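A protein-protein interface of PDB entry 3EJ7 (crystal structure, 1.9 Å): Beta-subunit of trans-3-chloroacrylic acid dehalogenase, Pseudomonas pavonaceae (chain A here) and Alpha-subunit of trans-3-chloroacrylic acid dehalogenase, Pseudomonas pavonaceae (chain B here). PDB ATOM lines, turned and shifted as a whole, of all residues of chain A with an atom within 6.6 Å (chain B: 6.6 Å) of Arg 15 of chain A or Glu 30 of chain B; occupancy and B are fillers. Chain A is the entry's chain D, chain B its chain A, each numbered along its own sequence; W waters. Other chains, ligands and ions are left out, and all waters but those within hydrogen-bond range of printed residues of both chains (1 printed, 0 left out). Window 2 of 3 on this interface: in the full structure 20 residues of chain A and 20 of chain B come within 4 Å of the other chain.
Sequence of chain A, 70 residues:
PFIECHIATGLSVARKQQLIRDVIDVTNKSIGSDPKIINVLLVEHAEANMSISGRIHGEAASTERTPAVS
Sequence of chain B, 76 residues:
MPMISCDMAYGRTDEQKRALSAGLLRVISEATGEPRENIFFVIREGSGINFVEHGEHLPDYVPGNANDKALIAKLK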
ATOM      1  N   LEU A  11      14.513  36.272   0.406  1.00  0.00           N
ATOM      2  CA  LEU A  11      13.190  35.691   0.110  1.00  0.00           C
ATOM      3  C   LEU A  11      12.095  36.311   0.970  1.00  0.00           C
ATOM      4  O   LEU A  11      12.334  36.689   2.103  1.00  0.00           O
ATOM      5  CB  LEU A  11      13.164  34.167   0.316  1.00  0.00           C
ATOM      6  CG  LEU A  11      14.195  33.244  -0.339  1.00  0.00           C
ATOM      7  CD1 LEU A  11      13.729  31.777  -0.242  1.00  0.00           C
ATOM      8  CD2 LEU A  11      14.493  33.659  -1.775  1.00  0.00           C
ATOM      9  N   SER A  12      10.874  36.350   0.443  1.00  0.00           N
ATOM     10  CA  SER A  12       9.701  36.757   1.224  1.00  0.00           C
ATOM     11  C   SER A  12       9.412  35.704   2.312  1.00  0.00           C
ATOM     12  O   SER A  12       9.859  34.549   2.207  1.00  0.00           O
ATOM     13  CB  SER A  12       8.489  36.908   0.299  1.00  0.00           C
ATOM     14  OG  SER A  12       8.105  35.662  -0.238  1.00  0.00           O
ATOM     15  N   VAL A  13       8.656  36.104   3.336  1.00  0.00           N
ATOM     16  CA  VAL A  13       8.236  35.214   4.418  1.00  0.00           C
ATOM     17  C   VAL A  13       7.390  34.070   3.824  1.00  0.00           C
ATOM     18  O   VAL A  13       7.513  32.886   4.213  1.00  0.00           O
ATOM     19  CB  VAL A  13       7.432  36.012   5.534  1.00  0.00           C
ATOM     20  CG1 VAL A  13       6.207  36.786   4.963  1.00  0.00           C
ATOM     21  CG2 VAL A  13       7.008  35.097   6.686  1.00  0.00           C
ATOM     22  N   ALA A  14       6.535  34.446   2.872  1.00  0.00           N
ATOM     23  CA  ALA A  14       5.680  33.503   2.169  1.00  0.00           C
ATOM     24  C   ALA A  14       6.494  32.449   1.405  1.00  0.00           C
ATOM     25  O   ALA A  14       6.116  31.268   1.363  1.00  0.00           O
ATOM     26  CB  ALA A  14       4.729  34.257   1.229  1.00  0.00           C
ATOM     27  N   ARG A  15       7.618  32.874   0.825  1.00  0.00           N
ATOM     28  CA  ARG A  15       8.451  32.002  -0.011  1.00  0.00           C
ATOM     29  C   ARG A  15       9.229  31.043   0.869  1.00  0.00           C
ATOM     30  O   ARG A  15       9.348  29.848   0.575  1.00  0.00           O
ATOM     31  CB  ARG A  15       9.394  32.831  -0.892  1.00  0.00           C
ATOM     32  CG  ARG A  15      10.155  32.053  -1.955  1.00  0.00           C
ATOM     33  CD  ARG A  15       9.226  31.671  -3.079  1.00  0.00           C
ATOM     34  NE  ARG A  15       9.933  31.355  -4.317  1.00  0.00           N
ATOM     35  CZ  ARG A  15      10.398  32.258  -5.183  1.00  0.00           C
ATOM     36  NH1 ARG A  15      11.015  31.845  -6.290  1.00  0.00           N
ATOM     37  NH2 ARG A  15      10.258  33.567  -4.949  1.00  0.00           N
ATOM     38  N   LYS A  16       9.741  31.558   1.973  1.00  0.00           N
ATOM     39  CA  LYS A  16      10.448  30.708   2.911  1.00  0.00           C
ATOM     40  C   LYS A  16       9.524  29.693   3.571  1.00  0.00           C
ATOM     41  O   LYS A  16       9.897  28.532   3.733  1.00  0.00           O
ATOM     42  CB  LYS A  16      11.197  31.539   3.927  1.00  0.00           C
ATOM     43  CG  LYS A  16      12.319  32.306   3.273  1.00  0.00           C
ATOM     44  CD  LYS A  16      13.303  32.877   4.272  1.00  0.00           C
ATOM     45  CE  LYS A  16      12.656  33.655   5.394  1.00  0.00           C
ATOM     46  NZ  LYS A  16      12.313  35.060   5.028  1.00  0.00           N
ATOM     47  N   GLN A  17       8.312  30.115   3.915  1.00  0.00           N
ATOM     48  CA  GLN A  17       7.321  29.188   4.480  1.00  0.00           C
ATOM     49  C   GLN A  17       6.981  28.033   3.510  1.00  0.00           C
ATOM     50  O   GLN A  17       6.910  26.857   3.917  1.00  0.00           O
ATOM     51  CB  GLN A  17       6.053  29.949   4.853  1.00  0.00           C
ATOM     52  CG  GLN A  17       4.946  29.037   5.303  1.00  0.00           C
ATOM     53  CD  GLN A  17       3.566  29.648   5.133  1.00  0.00           C
ATOM     54  OE1 GLN A  17       2.811  29.258   4.241  1.00  0.00           O
ATOM     55  NE2 GLN A  17       3.232  30.616   5.980  1.00  0.00           N
ATOM     56  N   GLN A  18       6.772  28.374   2.232  1.00  0.00           N
ATOM     57  CA  GLN A  18       6.596  27.346   1.211  1.00  0.00           C
ATOM     58  C   GLN A  18       7.798  26.413   1.082  1.00  0.00           C
ATOM     59  O   GLN A  18       7.628  25.211   0.870  1.00  0.00           O
ATOM     60  CB  GLN A  18       6.245  27.943  -0.160  1.00  0.00           C
ATOM     61  CG  GLN A  18       6.007  26.861  -1.196  1.00  0.00           C
ATOM     62  CD  GLN A  18       4.695  26.114  -0.960  1.00  0.00           C
ATOM     63  OE1 GLN A  18       3.658  26.729  -0.748  1.00  0.00           O
ATOM     64  NE2 GLN A  18       4.742  24.793  -0.996  1.00  0.00           N
ATOM     65  N   LEU A  19       9.002  26.974   1.178  1.00  0.00           N
ATOM     66  CA  LEU A  19      10.242  26.200   1.119  1.00  0.00           C
ATOM     67  C   LEU A  19      10.321  25.173   2.253  1.00  0.00           C
ATOM     68  O   LEU A  19      10.701  24.011   2.009  1.00  0.00           O
ATOM     69  CB  LEU A  19      11.478  27.124   1.140  1.00  0.00           C
ATOM     70  CG  LEU A  19      12.849  26.448   1.274  1.00  0.00           C
ATOM     71  CD1 LEU A  19      13.120  25.445   0.135  1.00  0.00           C
ATOM     72  CD2 LEU A  19      13.939  27.492   1.364  1.00  0.00           C
ATOM     73  N   ILE A  20       9.940  25.585   3.468  1.00  0.00           N
ATOM     74  CA  ILE A  20       9.918  24.674   4.618  1.00  0.00           C
ATOM     75  C   ILE A  20       8.853  23.581   4.400  1.00  0.00           C
ATOM     76  O   ILE A  20       9.105  22.411   4.681  1.00  0.00           O
ATOM     77  CB  ILE A  20       9.699  25.413   5.950  1.00  0.00           C
ATOM     78  CG1 ILE A  20      10.896  26.334   6.240  1.00  0.00           C
ATOM     79  CG2 ILE A  20       9.549  24.411   7.114  1.00  0.00           C
ATOM     80  CD1 ILE A  20      10.617  27.453   7.257  1.00  0.00           C
ATOM     81  N   ASP A  22       7.822  22.457   1.469  1.00  0.00           N
ATOM     82  CA  ASP A  22       8.395  21.617   0.406  1.00  0.00           C
ATOM     83  C   ASP A  22       9.534  20.671   0.921  1.00  0.00           C
ATOM     84  O   ASP A  22       9.571  19.492   0.516  1.00  0.00           O
ATOM     85  CB  ASP A  22       8.864  22.477  -0.784  1.00  0.00           C
ATOM     86  CG  ASP A  22       7.705  23.110  -1.578  1.00  0.00           C
ATOM     87  OD1 ASP A  22       7.989  23.806  -2.580  1.00  0.00           O
ATOM     88  OD2 ASP A  22       6.513  22.939  -1.223  1.00  0.00           O
ATOM     89  N   LEU A  42      15.786  26.953   8.784  1.00  0.00           N
ATOM     90  CA  LEU A  42      16.178  27.796   7.656  1.00  0.00           C
ATOM     91  C   LEU A  42      16.975  28.983   8.173  1.00  0.00           C
ATOM     92  O   LEU A  42      16.487  29.742   9.020  1.00  0.00           O
ATOM     93  CB  LEU A  42      14.935  28.227   6.887  1.00  0.00           C
ATOM     94  CG  LEU A  42      15.035  28.996   5.586  1.00  0.00           C
ATOM     95  CD1 LEU A  42      16.045  28.358   4.584  1.00  0.00           C
ATOM     96  CD2 LEU A  42      13.619  29.031   4.984  1.00  0.00           C
ATOM     97  N   LEU B  25      17.323  19.323  -3.596  1.00  0.00           N
ATOM     98  CA  LEU B  25      17.986  20.177  -4.589  1.00  0.00           C
ATOM     99  C   LEU B  25      16.986  20.924  -5.452  1.00  0.00           C
ATOM    100  O   LEU B  25      17.186  22.097  -5.750  1.00  0.00           O
ATOM    101  CB  LEU B  25      18.923  19.378  -5.500  1.00  0.00           C
ATOM    102  CG  LEU B  25      20.420  19.335  -5.173  1.00  0.00           C
ATOM    103  CD1 LEU B  25      21.139  20.504  -5.772  1.00  0.00           C
ATOM    104  CD2 LEU B  25      20.689  19.261  -3.704  1.00  0.00           C
ATOM    105  N   ARG B  26      15.919  20.240  -5.854  1.00  0.00           N
ATOM    106  CA  ARG B  26      14.895  20.858  -6.672  1.00  0.00           C
ATOM    107  C   ARG B  26      14.201  21.969  -5.895  1.00  0.00           C
ATOM    108  O   ARG B  26      14.075  23.082  -6.390  1.00  0.00           O
ATOM    109  CB  ARG B  26      13.866  19.829  -7.154  1.00  0.00           C
ATOM    110  CG  ARG B  26      12.823  20.395  -8.116  1.00  0.00           C
ATOM    111  CD  ARG B  26      11.674  19.418  -8.336  1.00  0.00           C
ATOM    112  NE  ARG B  26      10.582  19.595  -7.377  1.00  0.00           N
ATOM    113  CZ  ARG B  26      10.367  18.823  -6.310  1.00  0.00           C
ATOM    114  NH1 ARG B  26      11.162  17.787  -6.050  1.00  0.00           N
ATOM    115  NH2 ARG B  26       9.345  19.083  -5.497  1.00  0.00           N
ATOM    116  N   VAL B  27      13.763  21.669  -4.676  1.00  0.00           N
ATOM    117  CA  VAL B  27      12.970  22.647  -3.935  1.00  0.00           C
ATOM    118  C   VAL B  27      13.757  23.879  -3.500  1.00  0.00           C
ATOM    119  O   VAL B  27      13.243  24.987  -3.584  1.00  0.00           O
ATOM    120  CB  VAL B  27      12.107  22.019  -2.792  1.00  0.00           C
ATOM    121  CG1 VAL B  27      11.138  21.010  -3.392  1.00  0.00           C
ATOM    122  CG2 VAL B  27      12.943  21.383  -1.740  1.00  0.00           C
ATOM    123  N   ILE B  28      14.996  23.674  -3.041  1.00  0.00           N
ATOM    124  CA  ILE B  28      15.887  24.781  -2.680  1.00  0.00           C
ATOM    125  C   ILE B  28      16.246  25.584  -3.921  1.00  0.00           C
ATOM    126  O   ILE B  28      16.211  26.812  -3.904  1.00  0.00           O
ATOM    127  CB  ILE B  28      17.173  24.302  -1.962  1.00  0.00           C
ATOM    128  CG1 ILE B  28      16.885  23.917  -0.514  1.00  0.00           C
ATOM    129  CG2 ILE B  28      18.233  25.403  -1.915  1.00  0.00           C
ATOM    130  CD1 ILE B  28      16.326  22.549  -0.311  1.00  0.00           C
ATOM    131  N   SER B  29      16.567  24.879  -5.007  1.00  0.00           N
ATOM    132  CA  SER B  29      16.849  25.557  -6.277  1.00  0.00           C
ATOM    133  C   SER B  29      15.689  26.417  -6.773  1.00  0.00           C
ATOM    134  O   SER B  29      15.897  27.528  -7.273  1.00  0.00           O
ATOM    135  CB  SER B  29      17.208  24.535  -7.356  1.00  0.00           C
ATOM    136  OG  SER B  29      17.655  25.226  -8.499  1.00  0.00           O
ATOM    137  N   GLU B  30      14.471  25.889  -6.692  1.00  0.00           N
ATOM    138  CA  GLU B  30      13.310  26.628  -7.176  1.00  0.00           C
ATOM    139  C   GLU B  30      12.958  27.818  -6.275  1.00  0.00           C
ATOM    140  O   GLU B  30      12.491  28.843  -6.768  1.00  0.00           O
ATOM    141  CB  GLU B  30      12.095  25.728  -7.325  1.00  0.00           C
ATOM    142  CG  GLU B  30      11.012  26.367  -8.171  1.00  0.00           C
ATOM    143  CD  GLU B  30       9.774  25.512  -8.283  1.00  0.00           C
ATOM    144  OE1 GLU B  30       8.791  25.808  -7.567  1.00  0.00           O
ATOM    145  OE2 GLU B  30       9.790  24.544  -9.078  1.00  0.00           O
ATOM    146  N   ALA B  31      13.165  27.669  -4.968  1.00  0.00           N
ATOM    147  CA  ALA B  31      12.866  28.752  -4.020  1.00  0.00           C
ATOM    148  C   ALA B  31      13.901  29.879  -4.051  1.00  0.00           C
ATOM    149  O   ALA B  31      13.535  31.054  -4.030  1.00  0.00           O
ATOM    150  CB  ALA B  31      12.675  28.216  -2.598  1.00  0.00           C
ATOM    151  N   THR B  32      15.183  29.527  -4.124  1.00  0.00           N
ATOM    152  CA  THR B  32      16.259  30.532  -4.081  1.00  0.00           C
ATOM    153  C   THR B  32      16.552  31.056  -5.477  1.00  0.00           C
ATOM    154  O   THR B  32      17.082  32.149  -5.630  1.00  0.00           O
ATOM    155  CB  THR B  32      17.581  29.973  -3.510  1.00  0.00           C
ATOM    156  OG1 THR B  32      18.152  29.047  -4.454  1.00  0.00           O
ATOM    157  CG2 THR B  32      17.361  29.287  -2.147  1.00  0.00           C
ATOM    158  N   GLY B  33      16.216  30.261  -6.486  1.00  0.00           N
ATOM    159  CA  GLY B  33      16.555  30.571  -7.861  1.00  0.00           C
ATOM    160  C   GLY B  33      17.979  30.198  -8.239  1.00  0.00           C
ATOM    161  O   GLY B  33      18.416  30.491  -9.343  1.00  0.00           O
ATOM    162  N   GLU B  34      18.714  29.556  -7.332  1.00  0.00           N
ATOM    163  CA  GLU B  34      20.109  29.176  -7.586  1.00  0.00           C
ATOM    164  C   GLU B  34      20.175  27.857  -8.379  1.00  0.00           C
ATOM    165  O   GLU B  34      19.355  26.966  -8.148  1.00  0.00           O
ATOM    166  CB  GLU B  34      20.854  29.037  -6.260  1.00  0.00           C
ATOM    167  CG  GLU B  34      22.166  29.791  -6.183  1.00  0.00           C
ATOM    168  CD  GLU B  34      22.023  31.122  -5.501  1.00  0.00           C
ATOM    169  OE1 GLU B  34      22.030  32.159  -6.213  1.00  0.00           O
ATOM    170  OE2 GLU B  34      21.898  31.137  -4.249  1.00  0.00           O
ATOM    171  N   ILE B  39      24.170  24.267  -4.876  1.00  0.00           N
ATOM    172  CA  ILE B  39      23.611  23.801  -3.616  1.00  0.00           C
ATOM    173  C   ILE B  39      24.406  22.598  -3.121  1.00  0.00           C
ATOM    174  O   ILE B  39      24.362  21.539  -3.759  1.00  0.00           O
ATOM    175  CB  ILE B  39      22.129  23.383  -3.811  1.00  0.00           C
ATOM    176  CG1 ILE B  39      21.261  24.571  -4.229  1.00  0.00           C
ATOM    177  CG2 ILE B  39      21.584  22.754  -2.549  1.00  0.00           C
ATOM    178  CD1 ILE B  39      20.025  24.159  -4.966  1.00  0.00           C
HETATM  179  O   HOH W   1      10.102  29.573  -7.453  1.00  0.00           O
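NH1 of Arg 15 of chain A is in hydrogen-bond range of O of Glu 30 of chain B (3.4 Å).
O of Ala 31 of chain B is in hydrogen-bond range of NH1 of Arg 15 of chain A (3.5 Å).
The side-chain amino group of Lys 16 of chain A lies within hydrogen-bond range of the backbone carbonyl oxygen of Leu 11 of chain A, 3.3 Å away.
The side-chain hydroxyl (OG) of Ser 12 of chain A lies within hydrogen-bond range of the backbone NH (N) of Arg 15 of chain A, at 3.0 Å.
OD2 of Asp 22 of chain A is in hydrogen-bond range of NE2 of Gln 18 of chain A, 2.6 Å away.
Of the printed residues of chain B, Leu 11 of chain A touches Ala 31 (3.6 Å).
Of chain B, only Glu 30 (3.4 Å) and Ala 31 (3.5 Å) come within 4 Å of Arg 15 of chain A.
Of the printed residues of chain B, Leu 19 of chain A touches Val 27 and Ala 31.
Printed residues of chain B within 4 Å of Asp 22 of chain A: Val 27 (3.8 Å).
Printed residues of chain A within 4 Å of Val 27 of chain B: Leu 19 and Asp 22.
Of the printed residues of chain A, Ala 31 of chain B touches Leu 11, Arg 15 and Leu 19.
Ile 39 of chain B touches none of the printed residues of chain A.
The nearest residue of chain B that does not touch Arg 15 of chain A is Thr 32 of chain B (5.2 Å).
The nearest printed residue of chain B that does not touch Asp 22 of chain A is Glu 30 of chain B (5.4 Å).
Water W1 lies within hydrogen-bond range of O of Glu 30 of chain B (2.6 Å) and NH1 of Arg 15 of chain A (2.7 Å).
Hydrophobic or aromatic side chains of chain B within 4 Å of the printed part of chain A: Val 27 and Ala 31.
Of the 12 printed residues of chain A, 4 touch a printed residue of chain B.
Printed residues of chain A that touch a printed residue of chain B: Leu 11, Arg 15, Leu 19 and Asp 22.
Among the printed residues, merely in contact across the chains: Leu 11 of chain A with Ala 31 of chain B (3.6 Å), Leu 19 of chain A with Val 27 of chain B (3.7 Å), Asp 22 of chain A with Val 27 of chain B (3.8 Å) and Leu 19 of chain A with Ala 31 of chain B (3.9 Å).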
